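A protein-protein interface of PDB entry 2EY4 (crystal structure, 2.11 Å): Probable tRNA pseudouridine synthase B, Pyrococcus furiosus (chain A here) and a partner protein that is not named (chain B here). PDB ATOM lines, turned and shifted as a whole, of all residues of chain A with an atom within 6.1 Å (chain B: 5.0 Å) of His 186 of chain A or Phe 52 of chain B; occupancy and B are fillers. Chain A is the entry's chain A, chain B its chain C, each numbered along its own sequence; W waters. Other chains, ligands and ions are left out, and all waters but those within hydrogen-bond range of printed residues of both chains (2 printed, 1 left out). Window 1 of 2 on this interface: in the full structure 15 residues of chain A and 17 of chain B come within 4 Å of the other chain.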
ATOM      1  N   PHE A 132      -5.471  19.320  17.571  1.00  0.00           N
ATOM      2  CA  PHE A 132      -6.737  18.786  17.113  1.00  0.00           C
ATOM      3  C   PHE A 132      -6.681  17.300  16.795  1.00  0.00           C
ATOM      4  O   PHE A 132      -7.622  16.751  16.230  1.00  0.00           O
ATOM      5  CB  PHE A 132      -7.230  19.588  15.911  1.00  0.00           C
ATOM      6  CG  PHE A 132      -7.850  20.899  16.284  1.00  0.00           C
ATOM      7  CD1 PHE A 132      -9.235  21.046  16.295  1.00  0.00           C
ATOM      8  CD2 PHE A 132      -7.053  21.984  16.625  1.00  0.00           C
ATOM      9  CE1 PHE A 132      -9.821  22.265  16.635  1.00  0.00           C
ATOM     10  CE2 PHE A 132      -7.620  23.208  16.967  1.00  0.00           C
ATOM     11  CZ  PHE A 132      -9.010  23.355  16.972  1.00  0.00           C
ATOM     12  N   ILE A 136     -11.993  15.018  19.638  1.00  0.00           N
ATOM     13  CA  ILE A 136     -12.273  16.438  19.638  1.00  0.00           C
ATOM     14  C   ILE A 136     -13.769  16.704  19.659  1.00  0.00           C
ATOM     15  O   ILE A 136     -14.574  15.818  19.381  1.00  0.00           O
ATOM     16  CB  ILE A 136     -11.657  17.135  18.402  1.00  0.00           C
ATOM     17  CG1 ILE A 136     -12.298  16.594  17.119  1.00  0.00           C
ATOM     18  CG2 ILE A 136     -10.156  16.901  18.371  1.00  0.00           C
ATOM     19  CD1 ILE A 136     -12.006  17.438  15.900  1.00  0.00           C
ATOM     20  N   ILE A 137     -14.131  17.936  19.993  1.00  0.00           N
ATOM     21  CA  ILE A 137     -15.531  18.325  20.059  1.00  0.00           C
ATOM     22  C   ILE A 137     -15.897  19.043  18.781  1.00  0.00           C
ATOM     23  O   ILE A 137     -15.275  20.046  18.419  1.00  0.00           O
ATOM     24  CB  ILE A 137     -15.784  19.257  21.243  1.00  0.00           C
ATOM     25  CG1 ILE A 137     -15.316  18.575  22.532  1.00  0.00           C
ATOM     26  CG2 ILE A 137     -17.254  19.631  21.304  1.00  0.00           C
ATOM     27  CD1 ILE A 137     -15.324  19.482  23.750  1.00  0.00           C
ATOM     28  N   GLN A 138     -16.909  18.531  18.095  1.00  0.00           N
ATOM     29  CA  GLN A 138     -17.340  19.128  16.843  1.00  0.00           C
ATOM     30  C   GLN A 138     -18.848  18.996  16.685  1.00  0.00           C
ATOM     31  O   GLN A 138     -19.367  17.898  16.517  1.00  0.00           O
ATOM     32  CB  GLN A 138     -16.623  18.437  15.679  1.00  0.00           C
ATOM     33  CG  GLN A 138     -16.762  19.131  14.337  1.00  0.00           C
ATOM     34  CD  GLN A 138     -16.152  18.326  13.211  1.00  0.00           C
ATOM     35  OE1 GLN A 138     -16.690  17.293  12.807  1.00  0.00           O
ATOM     36  NE2 GLN A 138     -15.013  18.786  12.706  1.00  0.00           N
ATOM     37  N   ARG A 139     -19.549  20.119  16.751  1.00  0.00           N
ATOM     38  CA  ARG A 139     -20.998  20.123  16.596  1.00  0.00           C
ATOM     39  C   ARG A 139     -21.340  19.960  15.113  1.00  0.00           C
ATOM     40  O   ARG A 139     -20.645  20.497  14.251  1.00  0.00           O
ATOM     41  CB  ARG A 139     -21.572  21.434  17.138  1.00  0.00           C
ATOM     42  CG  ARG A 139     -23.047  21.632  16.870  1.00  0.00           C
ATOM     43  CD  ARG A 139     -23.578  22.850  17.591  1.00  0.00           C
ATOM     44  NE  ARG A 139     -22.712  24.009  17.403  1.00  0.00           N
ATOM     45  CZ  ARG A 139     -22.998  25.229  17.841  1.00  0.00           C
ATOM     46  NH1 ARG A 139     -24.134  25.448  18.491  1.00  0.00           N
ATOM     47  NH2 ARG A 139     -22.147  26.227  17.640  1.00  0.00           N
ATOM     48  N   ARG A 181     -14.379  20.780   6.871  1.00  0.00           N
ATOM     49  CA  ARG A 181     -14.686  22.204   6.813  1.00  0.00           C
ATOM     50  C   ARG A 181     -14.748  22.817   8.217  1.00  0.00           C
ATOM     51  O   ARG A 181     -14.175  23.883   8.464  1.00  0.00           O
ATOM     52  CB  ARG A 181     -16.014  22.416   6.089  1.00  0.00           C
ATOM     53  CG  ARG A 181     -16.322  23.853   5.752  1.00  0.00           C
ATOM     54  CD  ARG A 181     -17.756  23.973   5.278  1.00  0.00           C
ATOM     55  NE  ARG A 181     -18.186  25.363   5.161  1.00  0.00           N
ATOM     56  CZ  ARG A 181     -19.459  25.752   5.106  1.00  0.00           C
ATOM     57  NH1 ARG A 181     -20.436  24.854   5.159  1.00  0.00           N
ATOM     58  NH2 ARG A 181     -19.756  27.042   5.003  1.00  0.00           N
ATOM     59  N   SER A 182     -15.430  22.136   9.139  1.00  0.00           N
ATOM     60  CA  SER A 182     -15.550  22.625  10.513  1.00  0.00           C
ATOM     61  C   SER A 182     -14.194  22.604  11.187  1.00  0.00           C
ATOM     62  O   SER A 182     -13.815  23.542  11.891  1.00  0.00           O
ATOM     63  CB  SER A 182     -16.522  21.755  11.309  1.00  0.00           C
ATOM     64  OG  SER A 182     -17.798  21.775  10.707  1.00  0.00           O
ATOM     65  N   LEU A 183     -13.471  21.515  10.969  1.00  0.00           N
ATOM     66  CA  LEU A 183     -12.148  21.358  11.540  1.00  0.00           C
ATOM     67  C   LEU A 183     -11.274  22.559  11.188  1.00  0.00           C
ATOM     68  O   LEU A 183     -10.630  23.144  12.054  1.00  0.00           O
ATOM     69  CB  LEU A 183     -11.499  20.075  11.014  1.00  0.00           C
ATOM     70  CG  LEU A 183     -10.026  19.903  11.386  1.00  0.00           C
ATOM     71  CD1 LEU A 183      -9.886  19.889  12.899  1.00  0.00           C
ATOM     72  CD2 LEU A 183      -9.491  18.621  10.784  1.00  0.00           C
ATOM     73  N   ILE A 184     -11.258  22.926   9.912  1.00  0.00           N
ATOM     74  CA  ILE A 184     -10.442  24.048   9.475  1.00  0.00           C
ATOM     75  C   ILE A 184     -10.957  25.360  10.056  1.00  0.00           C
ATOM     76  O   ILE A 184     -10.165  26.203  10.478  1.00  0.00           O
ATOM     77  CB  ILE A 184     -10.374  24.118   7.928  1.00  0.00           C
ATOM     78  CG1 ILE A 184      -9.561  22.928   7.413  1.00  0.00           C
ATOM     79  CG2 ILE A 184      -9.742  25.443   7.474  1.00  0.00           C
ATOM     80  CD1 ILE A 184      -9.534  22.788   5.909  1.00  0.00           C
ATOM     81  N   HIS A 185     -12.276  25.528  10.090  1.00  0.00           N
ATOM     82  CA  HIS A 185     -12.857  26.737  10.650  1.00  0.00           C
ATOM     83  C   HIS A 185     -12.427  26.897  12.111  1.00  0.00           C
ATOM     84  O   HIS A 185     -12.080  27.992  12.555  1.00  0.00           O
ATOM     85  CB  HIS A 185     -14.383  26.685  10.583  1.00  0.00           C
ATOM     86  CG  HIS A 185     -15.055  27.812  11.308  1.00  0.00           C
ATOM     87  ND1 HIS A 185     -14.917  29.129  10.926  1.00  0.00           N
ATOM     88  CD2 HIS A 185     -15.856  27.820  12.399  1.00  0.00           C
ATOM     89  CE1 HIS A 185     -15.606  29.899  11.749  1.00  0.00           C
ATOM     90  NE2 HIS A 185     -16.185  29.130  12.652  1.00  0.00           N
ATOM     91  N   HIS A 186     -12.463  25.796  12.857  1.00  0.00           N
ATOM     92  CA  HIS A 186     -12.082  25.819  14.262  1.00  0.00           C
ATOM     93  C   HIS A 186     -10.603  26.139  14.419  1.00  0.00           C
ATOM     94  O   HIS A 186     -10.206  26.834  15.351  1.00  0.00           O
ATOM     95  CB  HIS A 186     -12.399  24.475  14.929  1.00  0.00           C
ATOM     96  CG  HIS A 186     -13.862  24.218  15.112  1.00  0.00           C
ATOM     97  ND1 HIS A 186     -14.758  25.216  15.432  1.00  0.00           N
ATOM     98  CD2 HIS A 186     -14.577  23.068  15.083  1.00  0.00           C
ATOM     99  CE1 HIS A 186     -15.959  24.691  15.596  1.00  0.00           C
ATOM    100  NE2 HIS A 186     -15.876  23.389  15.391  1.00  0.00           N
ATOM    101  N   ILE A 187      -9.787  25.609  13.518  1.00  0.00           N
ATOM    102  CA  ILE A 187      -8.361  25.878  13.567  1.00  0.00           C
ATOM    103  C   ILE A 187      -8.162  27.383  13.393  1.00  0.00           C
ATOM    104  O   ILE A 187      -7.308  27.979  14.046  1.00  0.00           O
ATOM    105  CB  ILE A 187      -7.621  25.109  12.456  1.00  0.00           C
ATOM    106  CG1 ILE A 187      -7.533  23.627  12.833  1.00  0.00           C
ATOM    107  CG2 ILE A 187      -6.227  25.682  12.254  1.00  0.00           C
ATOM    108  CD1 ILE A 187      -7.049  22.737  11.711  1.00  0.00           C
ATOM    109  N   GLY A 188      -8.984  27.984  12.532  1.00  0.00           N
ATOM    110  CA  GLY A 188      -8.910  29.411  12.273  1.00  0.00           C
ATOM    111  C   GLY A 188      -9.188  30.221  13.525  1.00  0.00           C
ATOM    112  O   GLY A 188      -8.537  31.237  13.783  1.00  0.00           O
ATOM    113  N   LEU A 189     -10.164  29.772  14.306  1.00  0.00           N
ATOM    114  CA  LEU A 189     -10.516  30.452  15.541  1.00  0.00           C
ATOM    115  C   LEU A 189      -9.396  30.260  16.542  1.00  0.00           C
ATOM    116  O   LEU A 189      -8.976  31.209  17.203  1.00  0.00           O
ATOM    117  CB  LEU A 189     -11.822  29.896  16.109  1.00  0.00           C
ATOM    118  CG  LEU A 189     -13.110  30.240  15.354  1.00  0.00           C
ATOM    119  CD1 LEU A 189     -14.297  29.585  16.051  1.00  0.00           C
ATOM    120  CD2 LEU A 189     -13.298  31.755  15.308  1.00  0.00           C
ATOM    121  N   ALA A 190      -8.905  29.029  16.646  1.00  0.00           N
ATOM    122  CA  ALA A 190      -7.820  28.725  17.572  1.00  0.00           C
ATOM    123  C   ALA A 190      -6.598  29.603  17.297  1.00  0.00           C
ATOM    124  O   ALA A 190      -5.884  29.983  18.229  1.00  0.00           O
ATOM    125  CB  ALA A 190      -7.444  27.260  17.473  1.00  0.00           C
ATOM    126  N   LEU A 191      -6.366  29.923  16.023  1.00  0.00           N
ATOM    127  CA  LEU A 191      -5.233  30.756  15.622  1.00  0.00           C
ATOM    128  C   LEU A 191      -5.606  32.241  15.618  1.00  0.00           C
ATOM    129  O   LEU A 191      -4.774  33.100  15.325  1.00  0.00           O
ATOM    130  CB  LEU A 191      -4.738  30.342  14.232  1.00  0.00           C
ATOM    131  CG  LEU A 191      -4.082  28.962  14.133  1.00  0.00           C
ATOM    132  CD1 LEU A 191      -3.928  28.576  12.682  1.00  0.00           C
ATOM    133  CD2 LEU A 191      -2.730  28.970  14.840  1.00  0.00           C
ATOM    134  N   ILE B  24     -11.945  33.880  22.356  1.00  0.00           N
ATOM    135  CA  ILE B  24     -11.490  32.505  22.480  1.00  0.00           C
ATOM    136  C   ILE B  24     -10.780  32.275  23.806  1.00  0.00           C
ATOM    137  O   ILE B  24      -9.880  33.019  24.191  1.00  0.00           O
ATOM    138  CB  ILE B  24     -10.540  32.106  21.317  1.00  0.00           C
ATOM    139  CG1 ILE B  24     -11.329  31.959  20.016  1.00  0.00           C
ATOM    140  CG2 ILE B  24      -9.870  30.770  21.618  1.00  0.00           C
ATOM    141  CD1 ILE B  24     -12.039  33.206  19.567  1.00  0.00           C
ATOM    142  N   ASP B  50     -19.878  28.448  20.911  1.00  0.00           N
ATOM    143  CA  ASP B  50     -19.233  27.285  20.328  1.00  0.00           C
ATOM    144  C   ASP B  50     -18.140  26.727  21.226  1.00  0.00           C
ATOM    145  O   ASP B  50     -17.496  27.465  21.972  1.00  0.00           O
ATOM    146  CB  ASP B  50     -18.655  27.652  18.959  1.00  0.00           C
ATOM    147  CG  ASP B  50     -18.381  26.435  18.093  1.00  0.00           C
ATOM    148  OD1 ASP B  50     -17.967  26.619  16.928  1.00  0.00           O
ATOM    149  OD2 ASP B  50     -18.581  25.299  18.576  1.00  0.00           O
ATOM    150  N   VAL B  51     -17.950  25.414  21.160  1.00  0.00           N
ATOM    151  CA  VAL B  51     -16.927  24.735  21.942  1.00  0.00           C
ATOM    152  C   VAL B  51     -16.222  23.771  20.998  1.00  0.00           C
ATOM    153  O   VAL B  51     -16.875  23.038  20.263  1.00  0.00           O
ATOM    154  CB  VAL B  51     -17.548  23.940  23.096  1.00  0.00           C
ATOM    155  CG1 VAL B  51     -16.450  23.357  23.966  1.00  0.00           C
ATOM    156  CG2 VAL B  51     -18.473  24.839  23.899  1.00  0.00           C
ATOM    157  N   PHE B  52     -14.896  23.755  21.020  1.00  0.00           N
ATOM    158  CA  PHE B  52     -14.170  22.884  20.109  1.00  0.00           C
ATOM    159  C   PHE B  52     -12.779  22.495  20.568  1.00  0.00           C
ATOM    160  O   PHE B  52     -12.346  22.844  21.661  1.00  0.00           O
ATOM    161  CB  PHE B  52     -14.057  23.553  18.741  1.00  0.00           C
ATOM    162  CG  PHE B  52     -13.466  24.932  18.790  1.00  0.00           C
ATOM    163  CD1 PHE B  52     -14.229  26.013  19.218  1.00  0.00           C
ATOM    164  CD2 PHE B  52     -12.153  25.153  18.394  1.00  0.00           C
ATOM    165  CE1 PHE B  52     -13.696  27.300  19.249  1.00  0.00           C
ATOM    166  CE2 PHE B  52     -11.604  26.440  18.419  1.00  0.00           C
ATOM    167  CZ  PHE B  52     -12.379  27.513  18.846  1.00  0.00           C
ATOM    168  N   GLY B  53     -12.078  21.770  19.705  1.00  0.00           N
ATOM    169  CA  GLY B  53     -10.735  21.338  20.028  1.00  0.00           C
ATOM    170  C   GLY B  53     -10.765  20.019  20.770  1.00  0.00           C
ATOM    171  O   GLY B  53     -11.818  19.375  20.843  1.00  0.00           O
ATOM    172  N   PRO B  54      -9.627  19.589  21.337  1.00  0.00           N
ATOM    173  CA  PRO B  54      -9.560  18.326  22.071  1.00  0.00           C
ATOM    174  C   PRO B  54     -10.447  18.319  23.315  1.00  0.00           C
ATOM    175  O   PRO B  54     -10.503  19.298  24.064  1.00  0.00           O
ATOM    176  CB  PRO B  54      -8.073  18.195  22.392  1.00  0.00           C
ATOM    177  CG  PRO B  54      -7.619  19.604  22.495  1.00  0.00           C
ATOM    178  CD  PRO B  54      -8.327  20.279  21.356  1.00  0.00           C
ATOM    179  N   PRO B  58     -10.352  21.767  25.670  1.00  0.00           N
ATOM    180  CA  PRO B  58     -11.088  22.479  24.620  1.00  0.00           C
ATOM    181  C   PRO B  58     -10.978  24.010  24.558  1.00  0.00           C
ATOM    182  O   PRO B  58     -10.561  24.662  25.516  1.00  0.00           O
ATOM    183  CB  PRO B  58     -12.527  22.022  24.850  1.00  0.00           C
ATOM    184  CG  PRO B  58     -12.585  21.843  26.326  1.00  0.00           C
ATOM    185  CD  PRO B  58     -11.280  21.150  26.638  1.00  0.00           C
ATOM    186  N   TYR B  59     -11.347  24.561  23.400  1.00  0.00           N
ATOM    187  CA  TYR B  59     -11.367  26.005  23.177  1.00  0.00           C
ATOM    188  C   TYR B  59     -12.833  26.385  23.277  1.00  0.00           C
ATOM    189  O   TYR B  59     -13.709  25.555  23.010  1.00  0.00           O
ATOM    190  CB  TYR B  59     -10.890  26.392  21.765  1.00  0.00           C
ATOM    191  CG  TYR B  59      -9.405  26.286  21.507  1.00  0.00           C
ATOM    192  CD1 TYR B  59      -8.838  25.092  21.069  1.00  0.00           C
ATOM    193  CD2 TYR B  59      -8.568  27.388  21.687  1.00  0.00           C
ATOM    194  CE1 TYR B  59      -7.478  24.995  20.809  1.00  0.00           C
ATOM    195  CE2 TYR B  59      -7.202  27.301  21.434  1.00  0.00           C
ATOM    196  CZ  TYR B  59      -6.665  26.105  20.995  1.00  0.00           C
ATOM    197  OH  TYR B  59      -5.320  26.008  20.726  1.00  0.00           O
ATOM    198  N   VAL B  60     -13.108  27.629  23.644  1.00  0.00           N
ATOM    199  CA  VAL B  60     -14.486  28.084  23.741  1.00  0.00           C
ATOM    200  C   VAL B  60     -14.612  29.446  23.075  1.00  0.00           C
ATOM    201  O   VAL B  60     -13.784  30.332  23.291  1.00  0.00           O
ATOM    202  CB  VAL B  60     -14.942  28.186  25.210  1.00  0.00           C
ATOM    203  CG1 VAL B  60     -16.403  28.623  25.278  1.00  0.00           C
ATOM    204  CG2 VAL B  60     -14.760  26.844  25.896  1.00  0.00           C
ATOM    205  N   ALA B  61     -15.645  29.603  22.257  1.00  0.00           N
ATOM    206  CA  ALA B  61     -15.881  30.859  21.558  1.00  0.00           C
ATOM    207  C   ALA B  61     -17.031  31.633  22.186  1.00  0.00           C
ATOM    208  O   ALA B  61     -18.205  31.282  22.029  1.00  0.00           O
ATOM    209  CB  ALA B  61     -16.177  30.597  20.085  1.00  0.00           C
HETATM  210  O   HOH W   1     -12.920  20.319  17.142  1.00  0.00           O
HETATM  211  O   HOH W   2     -17.997  28.800  15.198  1.00  0.00           O
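N of Ile 137 of chain A lies within hydrogen-bond range of O of Gly 53 of chain B (2.9 Å).
The side-chain carboxylate (OD2) of Asp 50 of chain B lies within salt-bridge range of the guanidinium group (NH2) of Arg 139 of chain A.
The backbone carbonyl oxygen (O) of Asp 50 of chain B lies within hydrogen-bond range of the backbone NH (N) of Ala 61 of chain B.
The backbone carbonyl oxygen of Phe 52 of chain B lies within hydrogen-bond range of the backbone NH of Tyr 59 of chain B (2.6 Å).
Phe 132 of chain A touches Phe 52 of chain B.
CE1 of Phe 132 of chain A touches CA of Gly 53 of chain B (3.6 Å).
Gly 53 of chain B touches Ile 136 of chain A.
Ile 137 of chain A touches Val 51 of chain B.
CA of Phe 52 of chain B touches O of Ile 137 of chain A, at 3.5 Å.
CE1 of His 186 of chain A touches OD1 of Asp 50 of chain B (3.1 Å).
O of His 186 of chain A touches CE2 of Phe 52 of chain B, 3.4 Å away.
Ile 24 of chain B touches Leu 189 of chain A.
CB of Leu 189 of chain A touches CZ of Phe 52 of chain B (3.7 Å).
Ala 190 of chain A touches Tyr 59 of chain B.
Of the printed residues of chain B, Ile 137 of chain A touches Val 51 (3.6 Å), Phe 52 (3.5 Å), Gly 53 (2.9 Å) and Pro 58 (3.9 Å).
Of chain B, only Asp 50 and Phe 52 come within 4 Å of His 186 of chain A.
Of the printed residues of chain A, Ile 24 of chain B touches Leu 189 (3.7 Å).
Printed residues of chain A within 4 Å of Val 51 of chain B: Ile 137.
Phe 52 of chain B touches four residues of chain A.
Of the printed residues of chain A, Gly 53 of chain B touches Phe 132 (3.6 Å), Ile 136 (3.2 Å) and Ile 137 (2.9 Å).
Of the printed residues of chain A, Pro 58 of chain B touches Ile 137.
The nearest residue of chain A that does not touch Phe 52 of chain B is Ala 190 of chain A (4.1 Å).
The nearest printed residue of chain B that does not touch Phe 132 of chain A is Tyr 59 of chain B (4.2 Å).
Of the 16 printed residues of chain A, 7 touch a printed residue of chain B.
Printed residues of chain A that touch a printed residue of chain B: Phe 132, Ile 136, Ile 137, Arg 139, His 186, Leu 189 and Ala 190.
Hydrophobic or aromatic side chains of chain A that line the printed part of chain B: Phe 132, Ile 136, Ile 137, His 186, Leu 189 and Ala 190.
Printed residues of chain B that touch a printed residue of chain A: Ile 24, Asp 50, Val 51, Phe 52, Gly 53, Pro 58 and Tyr 59.
Hydrophobic or aromatic side chains of chain B that line the printed part of chain A: Ile 24, Phe 52, Pro 58 and Tyr 59.
Among the printed residues, 13 pairs touch across the chains.
Among the printed residues, Asp or Glu carboxylates within 4 Å of a Lys or Arg side-chain nitrogen of the other chain: Arg 139 of chain A with Asp 50 of chain B (3.8 Å).
Water W1 bridges the backbone carbonyl oxygen (O) of Ile 137 of chain A (2.7 Å) and the backbone NH (N) of Gly 53 of chain B (3.1 Å).
Water W2 bridges OD1 of Asp 50 of chain B (2.8 Å) and NE2 of His 185 of chain A (3.1 Å).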
